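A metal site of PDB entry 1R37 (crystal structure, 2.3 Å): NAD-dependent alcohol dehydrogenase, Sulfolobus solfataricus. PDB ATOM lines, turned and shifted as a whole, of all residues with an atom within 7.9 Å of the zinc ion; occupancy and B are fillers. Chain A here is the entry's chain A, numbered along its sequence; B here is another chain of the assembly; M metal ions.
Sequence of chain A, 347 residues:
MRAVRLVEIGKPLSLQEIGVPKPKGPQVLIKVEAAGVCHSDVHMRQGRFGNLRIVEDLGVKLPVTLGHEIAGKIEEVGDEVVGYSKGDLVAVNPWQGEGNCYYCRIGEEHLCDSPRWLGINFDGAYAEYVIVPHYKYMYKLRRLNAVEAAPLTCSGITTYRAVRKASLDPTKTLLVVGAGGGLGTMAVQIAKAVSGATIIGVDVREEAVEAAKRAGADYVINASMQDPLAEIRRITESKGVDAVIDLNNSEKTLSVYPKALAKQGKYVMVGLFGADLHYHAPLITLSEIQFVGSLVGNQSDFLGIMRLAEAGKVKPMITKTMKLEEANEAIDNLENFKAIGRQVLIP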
ATOM      1  N   GLN A  96      15.973  22.969 -27.042  1.00  0.00           N
ATOM      2  CA  GLN A  96      15.725  21.564 -26.796  1.00  0.00           C
ATOM      3  C   GLN A  96      16.848  20.578 -27.056  1.00  0.00           C
ATOM      4  O   GLN A  96      17.623  20.718 -28.003  1.00  0.00           O
ATOM      5  CB  GLN A  96      14.470  21.154 -27.553  1.00  0.00           C
ATOM      6  CG  GLN A  96      13.276  22.012 -27.163  1.00  0.00           C
ATOM      7  CD  GLN A  96      11.989  21.602 -27.843  1.00  0.00           C
ATOM      8  OE1 GLN A  96      11.805  20.430 -28.187  1.00  0.00           O
ATOM      9  NE2 GLN A  96      11.078  22.554 -28.008  1.00  0.00           N
ATOM     10  N   GLY A  97      16.925  19.575 -26.193  1.00  0.00           N
ATOM     11  CA  GLY A  97      17.932  18.541 -26.316  1.00  0.00           C
ATOM     12  C   GLY A  97      17.264  17.204 -26.566  1.00  0.00           C
ATOM     13  O   GLY A  97      16.069  17.034 -26.257  1.00  0.00           O
ATOM     14  N   GLU A  98      18.016  16.253 -27.114  1.00  0.00           N
ATOM     15  CA  GLU A  98      17.493  14.938 -27.437  1.00  0.00           C
ATOM     16  C   GLU A  98      17.315  14.009 -26.228  1.00  0.00           C
ATOM     17  O   GLU A  98      16.645  12.983 -26.334  1.00  0.00           O
ATOM     18  CB  GLU A  98      18.379  14.286 -28.501  1.00  0.00           C
ATOM     19  CG  GLU A  98      19.877  14.378 -28.241  1.00  0.00           C
ATOM     20  CD  GLU A  98      20.336  13.497 -27.101  1.00  0.00           C
ATOM     21  OE1 GLU A  98      19.862  12.342 -27.052  1.00  0.00           O
ATOM     22  OE2 GLU A  98      21.172  13.934 -26.267  1.00  0.00           O
ATOM     23  N   GLY A  99      17.931  14.348 -25.099  1.00  0.00           N
ATOM     24  CA  GLY A  99      17.747  13.562 -23.882  1.00  0.00           C
ATOM     25  C   GLY A  99      18.700  12.437 -23.499  1.00  0.00           C
ATOM     26  O   GLY A  99      18.589  11.903 -22.397  1.00  0.00           O
ATOM     27  N   ASN A 100      19.652  12.092 -24.366  1.00  0.00           N
ATOM     28  CA  ASN A 100      20.561  10.978 -24.083  1.00  0.00           C
ATOM     29  C   ASN A 100      22.034  11.343 -23.871  1.00  0.00           C
ATOM     30  O   ASN A 100      22.755  10.608 -23.208  1.00  0.00           O
ATOM     31  CB  ASN A 100      20.461   9.932 -25.208  1.00  0.00           C
ATOM     32  CG  ASN A 100      21.326   8.711 -24.963  1.00  0.00           C
ATOM     33  OD1 ASN A 100      21.131   7.991 -23.973  1.00  0.00           O
ATOM     34  ND2 ASN A 100      22.277   8.473 -25.844  1.00  0.00           N
ATOM     35  N   CYS A 101      22.472  12.468 -24.424  1.00  0.00           N
ATOM     36  CA  CYS A 101      23.872  12.874 -24.270  1.00  0.00           C
ATOM     37  C   CYS A 101      24.177  13.289 -22.840  1.00  0.00           C
ATOM     38  O   CYS A 101      23.274  13.476 -22.028  1.00  0.00           O
ATOM     39  CB  CYS A 101      24.217  14.027 -25.215  1.00  0.00           C
ATOM     40  SG  CYS A 101      23.633  15.681 -24.696  1.00  0.00           S
ATOM     41  N   TYR A 102      25.464  13.434 -22.551  1.00  0.00           N
ATOM     42  CA  TYR A 102      25.973  13.829 -21.248  1.00  0.00           C
ATOM     43  C   TYR A 102      25.252  15.050 -20.675  1.00  0.00           C
ATOM     44  O   TYR A 102      24.804  15.035 -19.523  1.00  0.00           O
ATOM     45  CB  TYR A 102      27.469  14.141 -21.333  1.00  0.00           C
ATOM     46  CG  TYR A 102      28.059  14.636 -20.026  1.00  0.00           C
ATOM     47  CD1 TYR A 102      28.467  13.746 -19.037  1.00  0.00           C
ATOM     48  CD2 TYR A 102      28.147  16.002 -19.754  1.00  0.00           C
ATOM     49  CE1 TYR A 102      28.937  14.198 -17.812  1.00  0.00           C
ATOM     50  CE2 TYR A 102      28.616  16.466 -18.536  1.00  0.00           C
ATOM     51  CZ  TYR A 102      29.003  15.557 -17.562  1.00  0.00           C
ATOM     52  OH  TYR A 102      29.446  15.998 -16.339  1.00  0.00           O
ATOM     53  N   TYR A 103      25.177  16.111 -21.466  1.00  0.00           N
ATOM     54  CA  TYR A 103      24.569  17.351 -20.994  1.00  0.00           C
ATOM     55  C   TYR A 103      23.078  17.224 -20.717  1.00  0.00           C
ATOM     56  O   TYR A 103      22.582  17.820 -19.773  1.00  0.00           O
ATOM     57  CB  TYR A 103      24.884  18.476 -21.983  1.00  0.00           C
ATOM     58  CG  TYR A 103      26.360  18.826 -21.983  1.00  0.00           C
ATOM     59  CD1 TYR A 103      26.912  19.644 -20.993  1.00  0.00           C
ATOM     60  CD2 TYR A 103      27.234  18.234 -22.899  1.00  0.00           C
ATOM     61  CE1 TYR A 103      28.286  19.849 -20.899  1.00  0.00           C
ATOM     62  CE2 TYR A 103      28.615  18.432 -22.819  1.00  0.00           C
ATOM     63  CZ  TYR A 103      29.139  19.238 -21.815  1.00  0.00           C
ATOM     64  OH  TYR A 103      30.505  19.410 -21.722  1.00  0.00           O
ATOM     65  N   CYS A 104      22.377  16.437 -21.528  1.00  0.00           N
ATOM     66  CA  CYS A 104      20.955  16.236 -21.291  1.00  0.00           C
ATOM     67  C   CYS A 104      20.739  15.450 -19.998  1.00  0.00           C
ATOM     68  O   CYS A 104      19.809  15.745 -19.250  1.00  0.00           O
ATOM     69  CB  CYS A 104      20.323  15.463 -22.461  1.00  0.00           C
ATOM     70  SG  CYS A 104      20.011  16.483 -23.927  1.00  0.00           S
ATOM     71  N   ARG A 105      21.607  14.487 -19.729  1.00  0.00           N
ATOM     72  CA  ARG A 105      21.487  13.664 -18.532  1.00  0.00           C
ATOM     73  C   ARG A 105      21.739  14.406 -17.220  1.00  0.00           C
ATOM     74  O   ARG A 105      21.192  14.030 -16.182  1.00  0.00           O
ATOM     75  CB  ARG A 105      22.403  12.455 -18.617  1.00  0.00           C
ATOM     76  CG  ARG A 105      22.013  11.485 -19.702  1.00  0.00           C
ATOM     77  CD  ARG A 105      22.660  10.147 -19.480  1.00  0.00           C
ATOM     78  NE  ARG A 105      22.383   9.199 -20.561  1.00  0.00           N
ATOM     79  CZ  ARG A 105      22.624   7.895 -20.481  1.00  0.00           C
ATOM     80  NH1 ARG A 105      23.137   7.399 -19.364  1.00  0.00           N
ATOM     81  NH2 ARG A 105      22.379   7.111 -21.524  1.00  0.00           N
ATOM     82  N   GLU A 108      21.181  19.794 -18.367  1.00  0.00           N
ATOM     83  CA  GLU A 108      21.679  20.956 -19.094  1.00  0.00           C
ATOM     84  C   GLU A 108      21.281  20.806 -20.575  1.00  0.00           C
ATOM     85  O   GLU A 108      22.114  20.891 -21.485  1.00  0.00           O
ATOM     86  CB  GLU A 108      23.209  21.061 -18.946  1.00  0.00           C
ATOM     87  CG  GLU A 108      23.697  21.251 -17.497  1.00  0.00           C
ATOM     88  CD  GLU A 108      23.197  22.553 -16.851  1.00  0.00           C
ATOM     89  OE1 GLU A 108      23.023  23.552 -17.590  1.00  0.00           O
ATOM     90  OE2 GLU A 108      22.994  22.599 -15.620  1.00  0.00           O
ATOM     91  N   GLU A 109      19.990  20.578 -20.780  1.00  0.00           N
ATOM     92  CA  GLU A 109      19.402  20.355 -22.098  1.00  0.00           C
ATOM     93  C   GLU A 109      19.840  21.318 -23.205  1.00  0.00           C
ATOM     94  O   GLU A 109      19.977  20.918 -24.357  1.00  0.00           O
ATOM     95  CB  GLU A 109      17.873  20.417 -22.011  1.00  0.00           C
ATOM     96  CG  GLU A 109      17.221  19.265 -21.268  1.00  0.00           C
ATOM     97  CD  GLU A 109      17.140  19.469 -19.754  1.00  0.00           C
ATOM     98  OE1 GLU A 109      16.688  18.522 -19.087  1.00  0.00           O
ATOM     99  OE2 GLU A 109      17.522  20.539 -19.234  1.00  0.00           O
ATOM    100  N   HIS A 110      20.029  22.589 -22.859  1.00  0.00           N
ATOM    101  CA  HIS A 110      20.392  23.568 -23.869  1.00  0.00           C
ATOM    102  C   HIS A 110      21.816  23.360 -24.408  1.00  0.00           C
ATOM    103  O   HIS A 110      22.161  23.864 -25.473  1.00  0.00           O
ATOM    104  CB  HIS A 110      20.230  24.984 -23.309  1.00  0.00           C
ATOM    105  CG  HIS A 110      21.134  25.288 -22.162  1.00  0.00           C
ATOM    106  ND1 HIS A 110      21.113  24.567 -20.989  1.00  0.00           N
ATOM    107  CD2 HIS A 110      22.098  26.229 -22.012  1.00  0.00           C
ATOM    108  CE1 HIS A 110      22.036  25.056 -20.165  1.00  0.00           C
ATOM    109  NE2 HIS A 110      22.636  26.057 -20.763  1.00  0.00           N
ATOM    110  N   LEU A 111      22.625  22.598 -23.679  1.00  0.00           N
ATOM    111  CA  LEU A 111      23.995  22.317 -24.092  1.00  0.00           C
ATOM    112  C   LEU A 111      24.110  20.911 -24.696  1.00  0.00           C
ATOM    113  O   LEU A 111      25.168  20.290 -24.693  1.00  0.00           O
ATOM    114  CB  LEU A 111      24.958  22.458 -22.910  1.00  0.00           C
ATOM    115  CG  LEU A 111      25.076  23.872 -22.346  1.00  0.00           C
ATOM    116  CD1 LEU A 111      25.933  23.852 -21.084  1.00  0.00           C
ATOM    117  CD2 LEU A 111      25.691  24.795 -23.397  1.00  0.00           C
ATOM    118  N   CYS A 112      22.993  20.443 -25.223  1.00  0.00           N
ATOM    119  CA  CYS A 112      22.925  19.127 -25.854  1.00  0.00           C
ATOM    120  C   CYS A 112      23.911  19.022 -27.008  1.00  0.00           C
ATOM    121  O   CYS A 112      24.156  20.009 -27.711  1.00  0.00           O
ATOM    122  CB  CYS A 112      21.517  18.895 -26.374  1.00  0.00           C
ATOM    123  SG  CYS A 112      21.341  17.366 -27.330  1.00  0.00           S
ATOM    124  N   ASP A 113      24.476  17.828 -27.220  1.00  0.00           N
ATOM    125  CA  ASP A 113      25.410  17.610 -28.320  1.00  0.00           C
ATOM    126  C   ASP A 113      24.703  17.669 -29.683  1.00  0.00           C
ATOM    127  O   ASP A 113      25.329  17.955 -30.704  1.00  0.00           O
ATOM    128  CB  ASP A 113      26.127  16.252 -28.188  1.00  0.00           C
ATOM    129  CG  ASP A 113      27.077  16.207 -27.001  1.00  0.00           C
ATOM    130  OD1 ASP A 113      27.786  17.204 -26.753  1.00  0.00           O
ATOM    131  OD2 ASP A 113      27.108  15.159 -26.324  1.00  0.00           O
ATOM    132  N   SER A 114      23.404  17.385 -29.683  1.00  0.00           N
ATOM    133  CA  SER A 114      22.600  17.439 -30.907  1.00  0.00           C
ATOM    134  C   SER A 114      21.414  18.356 -30.629  1.00  0.00           C
ATOM    135  O   SER A 114      20.262  17.921 -30.632  1.00  0.00           O
ATOM    136  CB  SER A 114      22.095  16.044 -31.286  1.00  0.00           C
ATOM    137  OG  SER A 114      23.186  15.178 -31.546  1.00  0.00           O
ATOM    138  N   PRO A 115      21.683  19.641 -30.415  1.00  0.00           N
ATOM    139  CA  PRO A 115      20.667  20.644 -30.116  1.00  0.00           C
ATOM    140  C   PRO A 115      19.623  20.903 -31.198  1.00  0.00           C
ATOM    141  O   PRO A 115      19.912  20.895 -32.391  1.00  0.00           O
ATOM    142  CB  PRO A 115      21.489  21.892 -29.819  1.00  0.00           C
ATOM    143  CG  PRO A 115      22.619  21.758 -30.806  1.00  0.00           C
ATOM    144  CD  PRO A 115      22.993  20.294 -30.659  1.00  0.00           C
ATOM    145  N   TYR A 137       8.808  20.391 -23.364  1.00  0.00           N
ATOM    146  CA  TYR A 137       9.428  21.708 -23.328  1.00  0.00           C
ATOM    147  C   TYR A 137       8.392  22.833 -23.340  1.00  0.00           C
ATOM    148  O   TYR A 137       8.739  23.990 -23.577  1.00  0.00           O
ATOM    149  CB  TYR A 137      10.382  21.883 -24.516  1.00  0.00           C
ATOM    150  CG  TYR A 137      11.693  21.143 -24.363  1.00  0.00           C
ATOM    151  CD1 TYR A 137      12.751  21.710 -23.654  1.00  0.00           C
ATOM    152  CD2 TYR A 137      11.861  19.867 -24.893  1.00  0.00           C
ATOM    153  CE1 TYR A 137      13.956  21.024 -23.490  1.00  0.00           C
ATOM    154  CE2 TYR A 137      13.056  19.171 -24.744  1.00  0.00           C
ATOM    155  CZ  TYR A 137      14.100  19.753 -24.036  1.00  0.00           C
ATOM    156  OH  TYR A 137      15.281  19.072 -23.873  1.00  0.00           O
ATOM    157  N   LYS B 263      32.191  21.956 -23.022  1.00  0.00           N
ATOM    158  CA  LYS B 263      31.145  22.905 -22.668  1.00  0.00           C
ATOM    159  C   LYS B 263      31.040  22.912 -21.136  1.00  0.00           C
ATOM    160  O   LYS B 263      31.183  21.869 -20.498  1.00  0.00           O
ATOM    161  CB  LYS B 263      29.821  22.503 -23.328  1.00  0.00           C
ATOM    162  CG  LYS B 263      29.807  22.794 -24.819  1.00  0.00           C
ATOM    163  CD  LYS B 263      28.536  22.291 -25.493  1.00  0.00           C
ATOM    164  CE  LYS B 263      28.531  20.774 -25.600  1.00  0.00           C
ATOM    165  NZ  LYS B 263      27.305  20.297 -26.307  1.00  0.00           N
HETATM  166 ZN    ZN M   1      21.525  15.914 -25.569  1.00  0.00          ZN
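Residues that only touch the zinc ion: Asp 113 (3.9 Å) and Gly 99 (3.9 Å). Within 4 Å of the zinc ion: Glu 98, Gly 99, Cys 101, Cys 104, Cys 112 and Asp 113. Along chain A the residues within 4 Å of the zinc ion span positions 98 to 113. The nearest printed residue that does not touch the zinc ion is Asn 100 (4.4 Å).
OE1 of Glu 98 lies within hydrogen-bond range of N of Asn 100 (2.7 Å). SG of Cys 112 sits close to N of Ser 114 (3.1 Å). O of Cys 112 lies within hydrogen-bond range of NZ of Lys 263 of chain B, at 3.5 Å. The side-chain sulfur of Cys 101 sits close to the backbone NH of Asp 113 (3.4 Å). N of Tyr 103 sits close to SG of Cys 101, at 3.6 Å. The side-chain sulfur of Cys 104 lies close to the backbone NH of Gly 99 (3.2 Å). The side-chain carboxylate (OD1) of Asp 113 is in salt-bridge range of the side-chain amino group (NZ) of Lys 263 of chain B.
The zinc ion is bound by OE2 of Glu 98, SG of Cys 112, SG of Cys 101 and SG of Cys 104.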
